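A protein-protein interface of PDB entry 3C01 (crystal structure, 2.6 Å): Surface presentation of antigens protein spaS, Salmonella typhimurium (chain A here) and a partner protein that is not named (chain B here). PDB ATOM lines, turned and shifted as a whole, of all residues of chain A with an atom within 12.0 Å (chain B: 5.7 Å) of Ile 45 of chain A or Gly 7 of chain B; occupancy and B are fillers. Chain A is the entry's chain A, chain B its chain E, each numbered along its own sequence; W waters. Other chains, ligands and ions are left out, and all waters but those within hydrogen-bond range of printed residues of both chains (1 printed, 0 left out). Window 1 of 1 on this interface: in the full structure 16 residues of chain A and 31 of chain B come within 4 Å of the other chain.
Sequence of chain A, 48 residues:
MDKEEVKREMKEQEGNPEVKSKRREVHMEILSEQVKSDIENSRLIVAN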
ATOM      1  N   LEU A  31      -0.736  -6.046 -26.254  1.00  0.00           N
ATOM      2  CA  LEU A  31       0.600  -6.512 -26.578  1.00  0.00           C
ATOM      3  C   LEU A  31       0.701  -8.000 -26.303  1.00  0.00           C
ATOM      4  O   LEU A  31       0.390  -8.447 -25.229  1.00  0.00           O
ATOM      5  CB  LEU A  31       1.631  -5.788 -25.743  1.00  0.00           C
ATOM      6  CG  LEU A  31       1.822  -4.288 -25.884  1.00  0.00           C
ATOM      7  CD1 LEU A  31       2.929  -3.932 -24.915  1.00  0.00           C
ATOM      8  CD2 LEU A  31       2.218  -3.844 -27.314  1.00  0.00           C
ATOM      9  N   GLN A  34       4.850 -12.294 -27.201  1.00  0.00           N
ATOM     10  CA  GLN A  34       6.021 -12.099 -28.067  1.00  0.00           C
ATOM     11  C   GLN A  34       6.624 -10.681 -27.981  1.00  0.00           C
ATOM     12  O   GLN A  34       7.832 -10.501 -27.823  1.00  0.00           O
ATOM     13  CB  GLN A  34       5.681 -12.388 -29.509  1.00  0.00           C
ATOM     14  CG  GLN A  34       6.866 -12.207 -30.471  1.00  0.00           C
ATOM     15  CD  GLN A  34       7.992 -13.178 -30.208  1.00  0.00           C
ATOM     16  OE1 GLN A  34       7.778 -14.395 -30.173  1.00  0.00           O
ATOM     17  NE2 GLN A  34       9.209 -12.650 -30.067  1.00  0.00           N
ATOM     18  N   VAL A  35       5.788  -9.676 -28.120  1.00  0.00           N
ATOM     19  CA  VAL A  35       6.304  -8.298 -28.096  1.00  0.00           C
ATOM     20  C   VAL A  35       6.794  -7.907 -26.720  1.00  0.00           C
ATOM     21  O   VAL A  35       7.808  -7.191 -26.596  1.00  0.00           O
ATOM     22  CB  VAL A  35       5.259  -7.302 -28.575  1.00  0.00           C
ATOM     23  CG1 VAL A  35       5.817  -5.880 -28.559  1.00  0.00           C
ATOM     24  CG2 VAL A  35       4.827  -7.714 -30.015  1.00  0.00           C
ATOM     25  N   LYS A  36       6.099  -8.363 -25.680  1.00  0.00           N
ATOM     26  CA  LYS A  36       6.590  -8.136 -24.348  1.00  0.00           C
ATOM     27  C   LYS A  36       8.033  -8.634 -24.218  1.00  0.00           C
ATOM     28  O   LYS A  36       8.927  -7.929 -23.729  1.00  0.00           O
ATOM     29  CB  LYS A  36       5.680  -8.802 -23.331  1.00  0.00           C
ATOM     30  CG  LYS A  36       4.421  -7.952 -23.035  1.00  0.00           C
ATOM     31  CD  LYS A  36       3.370  -8.727 -22.327  1.00  0.00           C
ATOM     32  CE  LYS A  36       2.181  -7.872 -22.006  1.00  0.00           C
ATOM     33  NZ  LYS A  36       1.247  -8.572 -21.085  1.00  0.00           N
ATOM     34  N   SER A  37       8.259  -9.835 -24.707  1.00  0.00           N
ATOM     35  CA  SER A  37       9.562 -10.466 -24.644  1.00  0.00           C
ATOM     36  C   SER A  37      10.565  -9.635 -25.439  1.00  0.00           C
ATOM     37  O   SER A  37      11.697  -9.374 -24.988  1.00  0.00           O
ATOM     38  CB  SER A  37       9.429 -11.844 -25.227  1.00  0.00           C
ATOM     39  OG  SER A  37      10.666 -12.452 -25.331  1.00  0.00           O
ATOM     40  N   ASP A  38      10.135  -9.183 -26.609  1.00  0.00           N
ATOM     41  CA  ASP A  38      11.000  -8.397 -27.451  1.00  0.00           C
ATOM     42  C   ASP A  38      11.403  -7.092 -26.730  1.00  0.00           C
ATOM     43  O   ASP A  38      12.554  -6.696 -26.771  1.00  0.00           O
ATOM     44  CB  ASP A  38      10.329  -8.130 -28.804  1.00  0.00           C
ATOM     45  CG  ASP A  38      10.158  -9.422 -29.680  1.00  0.00           C
ATOM     46  OD1 ASP A  38      10.893 -10.425 -29.496  1.00  0.00           O
ATOM     47  OD2 ASP A  38       9.291  -9.436 -30.599  1.00  0.00           O
ATOM     48  N   ILE A  39      10.475  -6.453 -26.022  1.00  0.00           N
ATOM     49  CA  ILE A  39      10.794  -5.266 -25.227  1.00  0.00           C
ATOM     50  C   ILE A  39      11.768  -5.626 -24.132  1.00  0.00           C
ATOM     51  O   ILE A  39      12.787  -4.951 -23.955  1.00  0.00           O
ATOM     52  CB  ILE A  39       9.537  -4.633 -24.592  1.00  0.00           C
ATOM     53  CG1 ILE A  39       8.605  -4.079 -25.692  1.00  0.00           C
ATOM     54  CG2 ILE A  39       9.934  -3.557 -23.606  1.00  0.00           C
ATOM     55  CD1 ILE A  39       7.175  -3.869 -25.316  1.00  0.00           C
ATOM     56  N   GLU A  40      11.508  -6.716 -23.423  1.00  0.00           N
ATOM     57  CA  GLU A  40      12.383  -7.071 -22.319  1.00  0.00           C
ATOM     58  C   GLU A  40      13.827  -7.256 -22.775  1.00  0.00           C
ATOM     59  O   GLU A  40      14.760  -6.962 -22.056  1.00  0.00           O
ATOM     60  CB  GLU A  40      11.877  -8.315 -21.599  1.00  0.00           C
ATOM     61  CG  GLU A  40      10.677  -8.038 -20.751  1.00  0.00           C
ATOM     62  CD  GLU A  40       9.844  -9.292 -20.395  1.00  0.00           C
ATOM     63  OE1 GLU A  40      10.355 -10.433 -20.517  1.00  0.00           O
ATOM     64  OE2 GLU A  40       8.653  -9.120 -20.000  1.00  0.00           O
ATOM     65  N   ASN A  41      14.013  -7.707 -23.997  1.00  0.00           N
ATOM     66  CA  ASN A  41      15.347  -7.961 -24.509  1.00  0.00           C
ATOM     67  C   ASN A  41      15.978  -6.819 -25.271  1.00  0.00           C
ATOM     68  O   ASN A  41      17.072  -6.981 -25.823  1.00  0.00           O
ATOM     69  CB  ASN A  41      15.292  -9.211 -25.366  1.00  0.00           C
ATOM     70  CG  ASN A  41      15.301 -10.448 -24.527  1.00  0.00           C
ATOM     71  OD1 ASN A  41      16.349 -10.828 -24.021  1.00  0.00           O
ATOM     72  ND2 ASN A  41      14.143 -11.061 -24.335  1.00  0.00           N
ATOM     73  N   SER A  42      15.315  -5.663 -25.288  1.00  0.00           N
ATOM     74  CA  SER A  42      15.856  -4.518 -26.010  1.00  0.00           C
ATOM     75  C   SER A  42      16.772  -3.738 -25.090  1.00  0.00           C
ATOM     76  O   SER A  42      16.605  -3.790 -23.910  1.00  0.00           O
ATOM     77  CB  SER A  42      14.706  -3.635 -26.507  1.00  0.00           C
ATOM     78  OG  SER A  42      13.769  -4.397 -27.237  1.00  0.00           O
ATOM     79  N   ARG A  43      17.753  -3.041 -25.648  1.00  0.00           N
ATOM     80  CA  ARG A  43      18.582  -2.089 -24.913  1.00  0.00           C
ATOM     81  C   ARG A  43      17.785  -0.833 -24.653  1.00  0.00           C
ATOM     82  O   ARG A  43      17.868  -0.258 -23.581  1.00  0.00           O
ATOM     83  CB  ARG A  43      19.795  -1.643 -25.737  1.00  0.00           C
ATOM     84  CG  ARG A  43      21.167  -2.030 -25.216  1.00  0.00           C
ATOM     85  CD  ARG A  43      21.285  -1.664 -23.819  1.00  0.00           C
ATOM     86  NE  ARG A  43      22.538  -1.032 -23.447  1.00  0.00           N
ATOM     87  CZ  ARG A  43      22.732  -0.537 -22.226  1.00  0.00           C
ATOM     88  NH1 ARG A  43      21.761  -0.635 -21.326  1.00  0.00           N
ATOM     89  NH2 ARG A  43      23.877   0.053 -21.898  1.00  0.00           N
ATOM     90  N   LEU A  44      17.104  -0.353 -25.695  1.00  0.00           N
ATOM     91  CA  LEU A  44      16.245   0.784 -25.554  1.00  0.00           C
ATOM     92  C   LEU A  44      15.054   0.806 -26.476  1.00  0.00           C
ATOM     93  O   LEU A  44      14.999   0.088 -27.445  1.00  0.00           O
ATOM     94  CB  LEU A  44      17.037   2.072 -25.685  1.00  0.00           C
ATOM     95  CG  LEU A  44      17.619   2.693 -26.972  1.00  0.00           C
ATOM     96  CD1 LEU A  44      19.077   2.337 -27.102  1.00  0.00           C
ATOM     97  CD2 LEU A  44      16.848   2.423 -28.246  1.00  0.00           C
ATOM     98  N   ILE A  45      14.086   1.646 -26.149  1.00  0.00           N
ATOM     99  CA  ILE A  45      13.022   1.996 -27.086  1.00  0.00           C
ATOM    100  C   ILE A  45      13.185   3.451 -27.533  1.00  0.00           C
ATOM    101  O   ILE A  45      13.295   4.343 -26.700  1.00  0.00           O
ATOM    102  CB  ILE A  45      11.631   1.868 -26.447  1.00  0.00           C
ATOM    103  CG1 ILE A  45      11.430   0.453 -25.847  1.00  0.00           C
ATOM    104  CG2 ILE A  45      10.585   2.226 -27.479  1.00  0.00           C
ATOM    105  CD1 ILE A  45      11.600  -0.721 -26.859  1.00  0.00           C
ATOM    106  N   VAL A  46      13.193   3.690 -28.836  1.00  0.00           N
ATOM    107  CA  VAL A  46      13.196   5.046 -29.332  1.00  0.00           C
ATOM    108  C   VAL A  46      11.773   5.452 -29.671  1.00  0.00           C
ATOM    109  O   VAL A  46      11.131   4.743 -30.380  1.00  0.00           O
ATOM    110  CB  VAL A  46      14.040   5.173 -30.594  1.00  0.00           C
ATOM    111  CG1 VAL A  46      14.009   6.617 -31.073  1.00  0.00           C
ATOM    112  CG2 VAL A  46      15.415   4.800 -30.294  1.00  0.00           C
ATOM    113  N   ALA A  47      11.284   6.575 -29.186  1.00  0.00           N
ATOM    114  CA  ALA A  47       9.901   6.963 -29.402  1.00  0.00           C
ATOM    115  C   ALA A  47       9.817   8.387 -29.905  1.00  0.00           C
ATOM    116  O   ALA A  47      10.766   9.182 -29.760  1.00  0.00           O
ATOM    117  CB  ALA A  47       9.106   6.834 -28.109  1.00  0.00           C
ATOM    118  N   ASN A  48       8.670   8.696 -30.497  1.00  0.00           N
ATOM    119  CA  ASN A  48       8.291  10.079 -30.793  1.00  0.00           C
ATOM    120  C   ASN A  48       7.254  10.564 -29.784  1.00  0.00           C
ATOM    121  O   ASN A  48       6.819   9.855 -28.864  1.00  0.00           O
ATOM    122  CB  ASN A  48       7.665  10.215 -32.181  1.00  0.00           C
ATOM    123  CG  ASN A  48       6.228   9.673 -32.244  1.00  0.00           C
ATOM    124  OD1 ASN A  48       5.842   8.788 -31.468  1.00  0.00           O
ATOM    125  ND2 ASN A  48       5.446  10.186 -33.183  1.00  0.00           N
ATOM    126  OXT ASN A  48       6.770  11.694 -29.912  1.00  0.00           O
ATOM    127  N   THR B   5       7.000   3.720 -31.955  1.00  0.00           N
ATOM    128  CA  THR B   5       7.873   3.125 -30.931  1.00  0.00           C
ATOM    129  C   THR B   5       8.763   2.108 -31.612  1.00  0.00           C
ATOM    130  O   THR B   5       8.245   1.168 -32.172  1.00  0.00           O
ATOM    131  CB  THR B   5       6.942   2.532 -29.910  1.00  0.00           C
ATOM    132  OG1 THR B   5       7.033   3.271 -28.659  1.00  0.00           O
ATOM    133  CG2 THR B   5       7.075   1.076 -29.825  1.00  0.00           C
ATOM    134  N   ILE B   6      10.076   2.347 -31.674  1.00  0.00           N
ATOM    135  CA  ILE B   6      11.040   1.427 -32.304  1.00  0.00           C
ATOM    136  C   ILE B   6      11.998   0.879 -31.246  1.00  0.00           C
ATOM    137  O   ILE B   6      12.552   1.644 -30.486  1.00  0.00           O
ATOM    138  CB  ILE B   6      11.906   2.145 -33.351  1.00  0.00           C
ATOM    139  CG1 ILE B   6      11.036   2.803 -34.454  1.00  0.00           C
ATOM    140  CG2 ILE B   6      12.888   1.188 -34.011  1.00  0.00           C
ATOM    141  CD1 ILE B   6      10.315   1.840 -35.379  1.00  0.00           C
ATOM    142  N   GLY B   7      12.176  -0.438 -31.172  1.00  0.00           N
ATOM    143  CA  GLY B   7      13.002  -1.041 -30.138  1.00  0.00           C
ATOM    144  C   GLY B   7      14.329  -1.435 -30.751  1.00  0.00           C
ATOM    145  O   GLY B   7      14.351  -1.884 -31.897  1.00  0.00           O
ATOM    146  N   ILE B   8      15.422  -1.238 -30.000  1.00  0.00           N
ATOM    147  CA  ILE B   8      16.756  -1.609 -30.431  1.00  0.00           C
ATOM    148  C   ILE B   8      17.304  -2.710 -29.549  1.00  0.00           C
ATOM    149  O   ILE B   8      17.400  -2.543 -28.326  1.00  0.00           O
ATOM    150  CB  ILE B   8      17.740  -0.413 -30.342  1.00  0.00           C
ATOM    151  CG1 ILE B   8      17.255   0.790 -31.191  1.00  0.00           C
ATOM    152  CG2 ILE B   8      19.196  -0.869 -30.695  1.00  0.00           C
ATOM    153  CD1 ILE B   8      17.139   0.526 -32.690  1.00  0.00           C
ATOM    154  N   TYR B   9      17.661  -3.830 -30.178  1.00  0.00           N
ATOM    155  CA  TYR B   9      18.341  -4.930 -29.506  1.00  0.00           C
ATOM    156  C   TYR B   9      19.809  -4.774 -29.852  1.00  0.00           C
ATOM    157  O   TYR B   9      20.162  -4.600 -31.030  1.00  0.00           O
ATOM    158  CB  TYR B   9      17.788  -6.263 -30.009  1.00  0.00           C
ATOM    159  CG  TYR B   9      18.590  -7.518 -29.703  1.00  0.00           C
ATOM    160  CD1 TYR B   9      19.752  -7.828 -30.416  1.00  0.00           C
ATOM    161  CD2 TYR B   9      18.149  -8.436 -28.755  1.00  0.00           C
ATOM    162  CE1 TYR B   9      20.468  -8.998 -30.164  1.00  0.00           C
ATOM    163  CE2 TYR B   9      18.860  -9.607 -28.487  1.00  0.00           C
ATOM    164  CZ  TYR B   9      20.018  -9.881 -29.199  1.00  0.00           C
ATOM    165  OH  TYR B   9      20.735 -11.019 -28.952  1.00  0.00           O
ATOM    166  N   MET B  19      19.723  -4.491 -33.790  1.00  0.00           N
ATOM    167  CA  MET B  19      18.560  -4.956 -34.511  1.00  0.00           C
ATOM    168  C   MET B  19      17.286  -4.236 -34.044  1.00  0.00           C
ATOM    169  O   MET B  19      17.185  -3.801 -32.909  1.00  0.00           O
ATOM    170  CB  MET B  19      18.416  -6.442 -34.270  1.00  0.00           C
ATOM    171  CG  MET B  19      17.155  -7.056 -34.762  1.00  0.00           C
ATOM    172  SD  MET B  19      17.123  -8.848 -34.438  1.00  0.00           S
ATOM    173  CE  MET B  19      16.035  -8.887 -32.992  1.00  0.00           C
ATOM    174  N   ILE B  20      16.325  -4.130 -34.950  1.00  0.00           N
ATOM    175  CA  ILE B  20      15.034  -3.587 -34.650  1.00  0.00           C
ATOM    176  C   ILE B  20      14.215  -4.681 -33.975  1.00  0.00           C
ATOM    177  O   ILE B  20      13.727  -5.588 -34.668  1.00  0.00           O
ATOM    178  CB  ILE B  20      14.284  -3.171 -35.900  1.00  0.00           C
ATOM    179  CG1 ILE B  20      15.112  -2.203 -36.796  1.00  0.00           C
ATOM    180  CG2 ILE B  20      12.998  -2.554 -35.504  1.00  0.00           C
ATOM    181  CD1 ILE B  20      15.520  -0.893 -36.153  1.00  0.00           C
ATOM    182  N   SER B  21      14.087  -4.591 -32.644  1.00  0.00           N
ATOM    183  CA  SER B  21      13.427  -5.585 -31.847  1.00  0.00           C
ATOM    184  C   SER B  21      11.929  -5.392 -31.773  1.00  0.00           C
ATOM    185  O   SER B  21      11.204  -6.350 -31.594  1.00  0.00           O
ATOM    186  CB  SER B  21      14.012  -5.573 -30.421  1.00  0.00           C
ATOM    187  OG  SER B  21      14.119  -4.250 -29.897  1.00  0.00           O
ATOM    188  N   VAL B  22      11.482  -4.136 -31.828  1.00  0.00           N
ATOM    189  CA  VAL B  22      10.096  -3.763 -31.613  1.00  0.00           C
ATOM    190  C   VAL B  22       9.742  -2.756 -32.684  1.00  0.00           C
ATOM    191  O   VAL B  22      10.553  -1.885 -32.995  1.00  0.00           O
ATOM    192  CB  VAL B  22       9.935  -3.098 -30.266  1.00  0.00           C
ATOM    193  CG1 VAL B  22       8.509  -2.551 -30.089  1.00  0.00           C
ATOM    194  CG2 VAL B  22      10.331  -4.070 -29.167  1.00  0.00           C
ATOM    195  N   TYR B  23       8.536  -2.869 -33.252  1.00  0.00           N
ATOM    196  CA  TYR B  23       8.096  -1.911 -34.266  1.00  0.00           C
ATOM    197  C   TYR B  23       6.569  -1.759 -34.205  1.00  0.00           C
ATOM    198  O   TYR B  23       5.842  -2.681 -34.583  1.00  0.00           O
ATOM    199  CB  TYR B  23       8.536  -2.444 -35.612  1.00  0.00           C
ATOM    200  CG  TYR B  23       8.363  -1.528 -36.796  1.00  0.00           C
ATOM    201  CD1 TYR B  23       9.433  -0.758 -37.249  1.00  0.00           C
ATOM    202  CD2 TYR B  23       7.177  -1.496 -37.508  1.00  0.00           C
ATOM    203  CE1 TYR B  23       9.326   0.056 -38.342  1.00  0.00           C
ATOM    204  CE2 TYR B  23       7.038  -0.663 -38.618  1.00  0.00           C
ATOM    205  CZ  TYR B  23       8.126   0.101 -39.031  1.00  0.00           C
ATOM    206  OH  TYR B  23       8.059   0.902 -40.144  1.00  0.00           O
ATOM    207  N   VAL B  32       3.570  -0.083 -25.774  1.00  0.00           N
ATOM    208  CA  VAL B  32       4.989  -0.431 -25.716  1.00  0.00           C
ATOM    209  C   VAL B  32       5.726   0.447 -24.747  1.00  0.00           C
ATOM    210  O   VAL B  32       6.470  -0.053 -23.941  1.00  0.00           O
ATOM    211  CB  VAL B  32       5.670  -0.350 -27.126  1.00  0.00           C
ATOM    212  CG1 VAL B  32       7.170  -0.412 -27.006  1.00  0.00           C
ATOM    213  CG2 VAL B  32       5.176  -1.499 -28.023  1.00  0.00           C
ATOM    214  N   ALA B  36       7.645  -0.862 -21.399  1.00  0.00           N
ATOM    215  CA  ALA B  36       9.051  -0.617 -21.163  1.00  0.00           C
ATOM    216  C   ALA B  36       9.304   0.154 -19.821  1.00  0.00           C
ATOM    217  O   ALA B  36      10.247  -0.163 -19.064  1.00  0.00           O
ATOM    218  CB  ALA B  36       9.571   0.146 -22.274  1.00  0.00           C
ATOM    219  N   VAL B  41      12.901  -0.742 -19.105  1.00  0.00           N
ATOM    220  CA  VAL B  41      13.722  -0.631 -20.317  1.00  0.00           C
ATOM    221  C   VAL B  41      13.656   0.810 -20.776  1.00  0.00           C
ATOM    222  O   VAL B  41      12.581   1.288 -21.019  1.00  0.00           O
ATOM    223  CB  VAL B  41      13.227  -1.511 -21.494  1.00  0.00           C
ATOM    224  CG1 VAL B  41      13.848  -1.013 -22.777  1.00  0.00           C
ATOM    225  CG2 VAL B  41      13.529  -3.012 -21.282  1.00  0.00           C
ATOM    226  N   PRO B  42      14.806   1.504 -20.894  1.00  0.00           N
ATOM    227  CA  PRO B  42      14.807   2.974 -21.166  1.00  0.00           C
ATOM    228  C   PRO B  42      14.133   3.418 -22.430  1.00  0.00           C
ATOM    229  O   PRO B  42      14.283   2.759 -23.460  1.00  0.00           O
ATOM    230  CB  PRO B  42      16.290   3.343 -21.242  1.00  0.00           C
ATOM    231  CG  PRO B  42      17.069   2.044 -21.036  1.00  0.00           C
ATOM    232  CD  PRO B  42      16.153   0.953 -20.663  1.00  0.00           C
ATOM    233  N   VAL B  43      13.432   4.550 -22.345  1.00  0.00           N
ATOM    234  CA  VAL B  43      12.677   5.138 -23.435  1.00  0.00           C
ATOM    235  C   VAL B  43      13.295   6.474 -23.802  1.00  0.00           C
ATOM    236  O   VAL B  43      13.407   7.347 -22.970  1.00  0.00           O
ATOM    237  CB  VAL B  43      11.192   5.328 -23.047  1.00  0.00           C
ATOM    238  CG1 VAL B  43      10.383   5.955 -24.222  1.00  0.00           C
ATOM    239  CG2 VAL B  43      10.562   3.988 -22.624  1.00  0.00           C
ATOM    240  N   ILE B  44      13.703   6.637 -25.052  1.00  0.00           N
ATOM    241  CA  ILE B  44      14.351   7.857 -25.501  1.00  0.00           C
ATOM    242  C   ILE B  44      13.458   8.542 -26.473  1.00  0.00           C
ATOM    243  O   ILE B  44      13.176   7.999 -27.508  1.00  0.00           O
ATOM    244  CB  ILE B  44      15.676   7.523 -26.157  1.00  0.00           C
ATOM    245  CG1 ILE B  44      16.566   6.839 -25.112  1.00  0.00           C
ATOM    246  CG2 ILE B  44      16.372   8.777 -26.631  1.00  0.00           C
ATOM    247  CD1 ILE B  44      17.899   6.434 -25.670  1.00  0.00           C
ATOM    248  N   VAL B  45      12.983   9.730 -26.147  1.00  0.00           N
ATOM    249  CA  VAL B  45      12.032  10.381 -27.017  1.00  0.00           C
ATOM    250  C   VAL B  45      12.816  11.253 -27.988  1.00  0.00           C
ATOM    251  O   VAL B  45      13.202  12.388 -27.674  1.00  0.00           O
ATOM    252  CB  VAL B  45      10.924  11.162 -26.263  1.00  0.00           C
ATOM    253  CG1 VAL B  45       9.842  11.591 -27.286  1.00  0.00           C
ATOM    254  CG2 VAL B  45      10.279  10.302 -25.161  1.00  0.00           C
HETATM  255  O   HOH W   1       8.419  -6.937 -31.377  1.00  0.00           O
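Of the printed residues of chain B, Ile 45 of chain A touches Thr 5, Ile 6, Gly 7, Pro 42, Val 43 and Ile 44. Ile 6 of chain B touches two residues of chain A. No residue of chain A comes within 4 Å of Met 19 of chain B. Ile 20 of chain B touches none of the printed residues of chain A. Val 22 of chain B touches just these residues of chain A: Ile 39 (3.9 Å) and Ser 42 (3.96 Å). Val 32 of chain B touches just these residues of chain A: Leu 31 and Ile 39. Ala 36 of chain B touches just one residue of chain A: Ile 39 (3.9 Å). Of chain A, only Ile 39 comes within 4 Å of Val 41 of chain B. Val 43 of chain B touches just one residue of chain A: Ile 45 (3.4 Å). Of chain A, only Leu 44 (3.97 Å), Ile 45 (2.9 Å), Val 46 (3.5 Å) and Ala 47 (2.9 Å) come within 4 Å of Ile 44 of chain B. Of the printed residues of chain B, Leu 31 of chain A touches Val 32. Of the printed residues of chain B, Asn 41 of chain A touches Tyr 9 (3.4 Å). Of the printed residues of chain B, Leu 44 of chain A touches Gly 7, Ile 8, Pro 42 and Ile 44. Of the printed residues of chain B, Ile 39 of chain A touches Val 22 (3.9 Å), Val 32 (3.8 Å), Ala 36 (3.9 Å) and Val 41 (3.4 Å). The nearest residue of chain B that does not touch Ile 45 of chain A is Ala 36 of chain B (4.04 Å).
NE2 of Gln 34 of chain A is in hydrogen-bond range of OD1 of Asp 38 of chain A (2.8 Å). The backbone carbonyl oxygen of Ile 39 of chain A sits close to the side-chain hydroxyl of Ser 42 of chain A, 3.5 Å away. N of Ser 21 of chain B is in hydrogen-bond range of O of Gly 7 of chain B. The backbone NH (N) of Gly 7 of chain B is in hydrogen-bond range of the backbone carbonyl oxygen (O) of Val 22 of chain B. The backbone NH of Tyr 9 of chain B sits at hydrogen-bond distance from the backbone carbonyl oxygen of Met 19 of chain B, at 2.8 Å. O of Ala 36 of chain B lies within hydrogen-bond range of N of Val 41 of chain B, 2.7 Å away.
Water W1 lies within hydrogen-bond range of OD2 of Asp 38 of chain A (2.8 Å) and O of Ser 21 of chain B (2.9 Å).
The side-chain hydroxyl (OG) of Ser 42 of chain A sits at hydrogen-bond distance from the side-chain hydroxyl (OG) of Ser 21 of chain B, at 2.7 Å. O of Ile 8 of chain B sits at hydrogen-bond distance from N of Arg 43 of chain A, 2.7 Å away. O of Leu 44 of chain A is in hydrogen-bond range of N of Ile 8 of chain B (2.9 Å). The backbone carbonyl oxygen of Pro 42 of chain B sits at hydrogen-bond distance from the backbone NH of Ile 45 of chain A. The backbone carbonyl oxygen (O) of Ile 45 of chain A is in hydrogen-bond range of the backbone NH (N) of Ile 44 of chain B (2.9 Å). N of Val 46 of chain A is in hydrogen-bond range of O of Ile 6 of chain B, at 2.7 Å. The backbone carbonyl oxygen (O) of Ile 44 of chain B lies within hydrogen-bond range of the backbone NH (N) of Ala 47 of chain A (2.9 Å).
Hydrophobic or aromatic side chains of chain B within 4 Å of the printed part of chain A: Ile 8, Tyr 9, Val 22, Val 32, Ala 36, Val 41, Pro 42, Ile 44 and Val 45. Of the 16 printed residues of chain A, 11 touch a printed residue of chain B.
Leu 31 of chain A touches Val 32 of chain B. Ser 21 of chain B touches Asp 38 of chain A. CD1 of Ile 39 of chain A touches CG1 of Val 32 of chain B (3.8 Å). Asn 41 of chain A touches Tyr 9 of chain B (O to CD2, 3.4 Å). CA of Ser 42 of chain A touches O of Ile 8 of chain B (3.4 Å). CA of Leu 44 of chain A touches O of Pro 42 of chain B, 3.5 Å away. CA of Ile 45 of chain A touches O of Ile 6 of chain B, at 3.5 Å. Ile 45 of chain A touches Gly 7 of chain B. Thr 5 of chain B touches Val 46 of chain A (CA to O, 3.7 Å). Asn 48 of chain A touches Val 45 of chain B.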
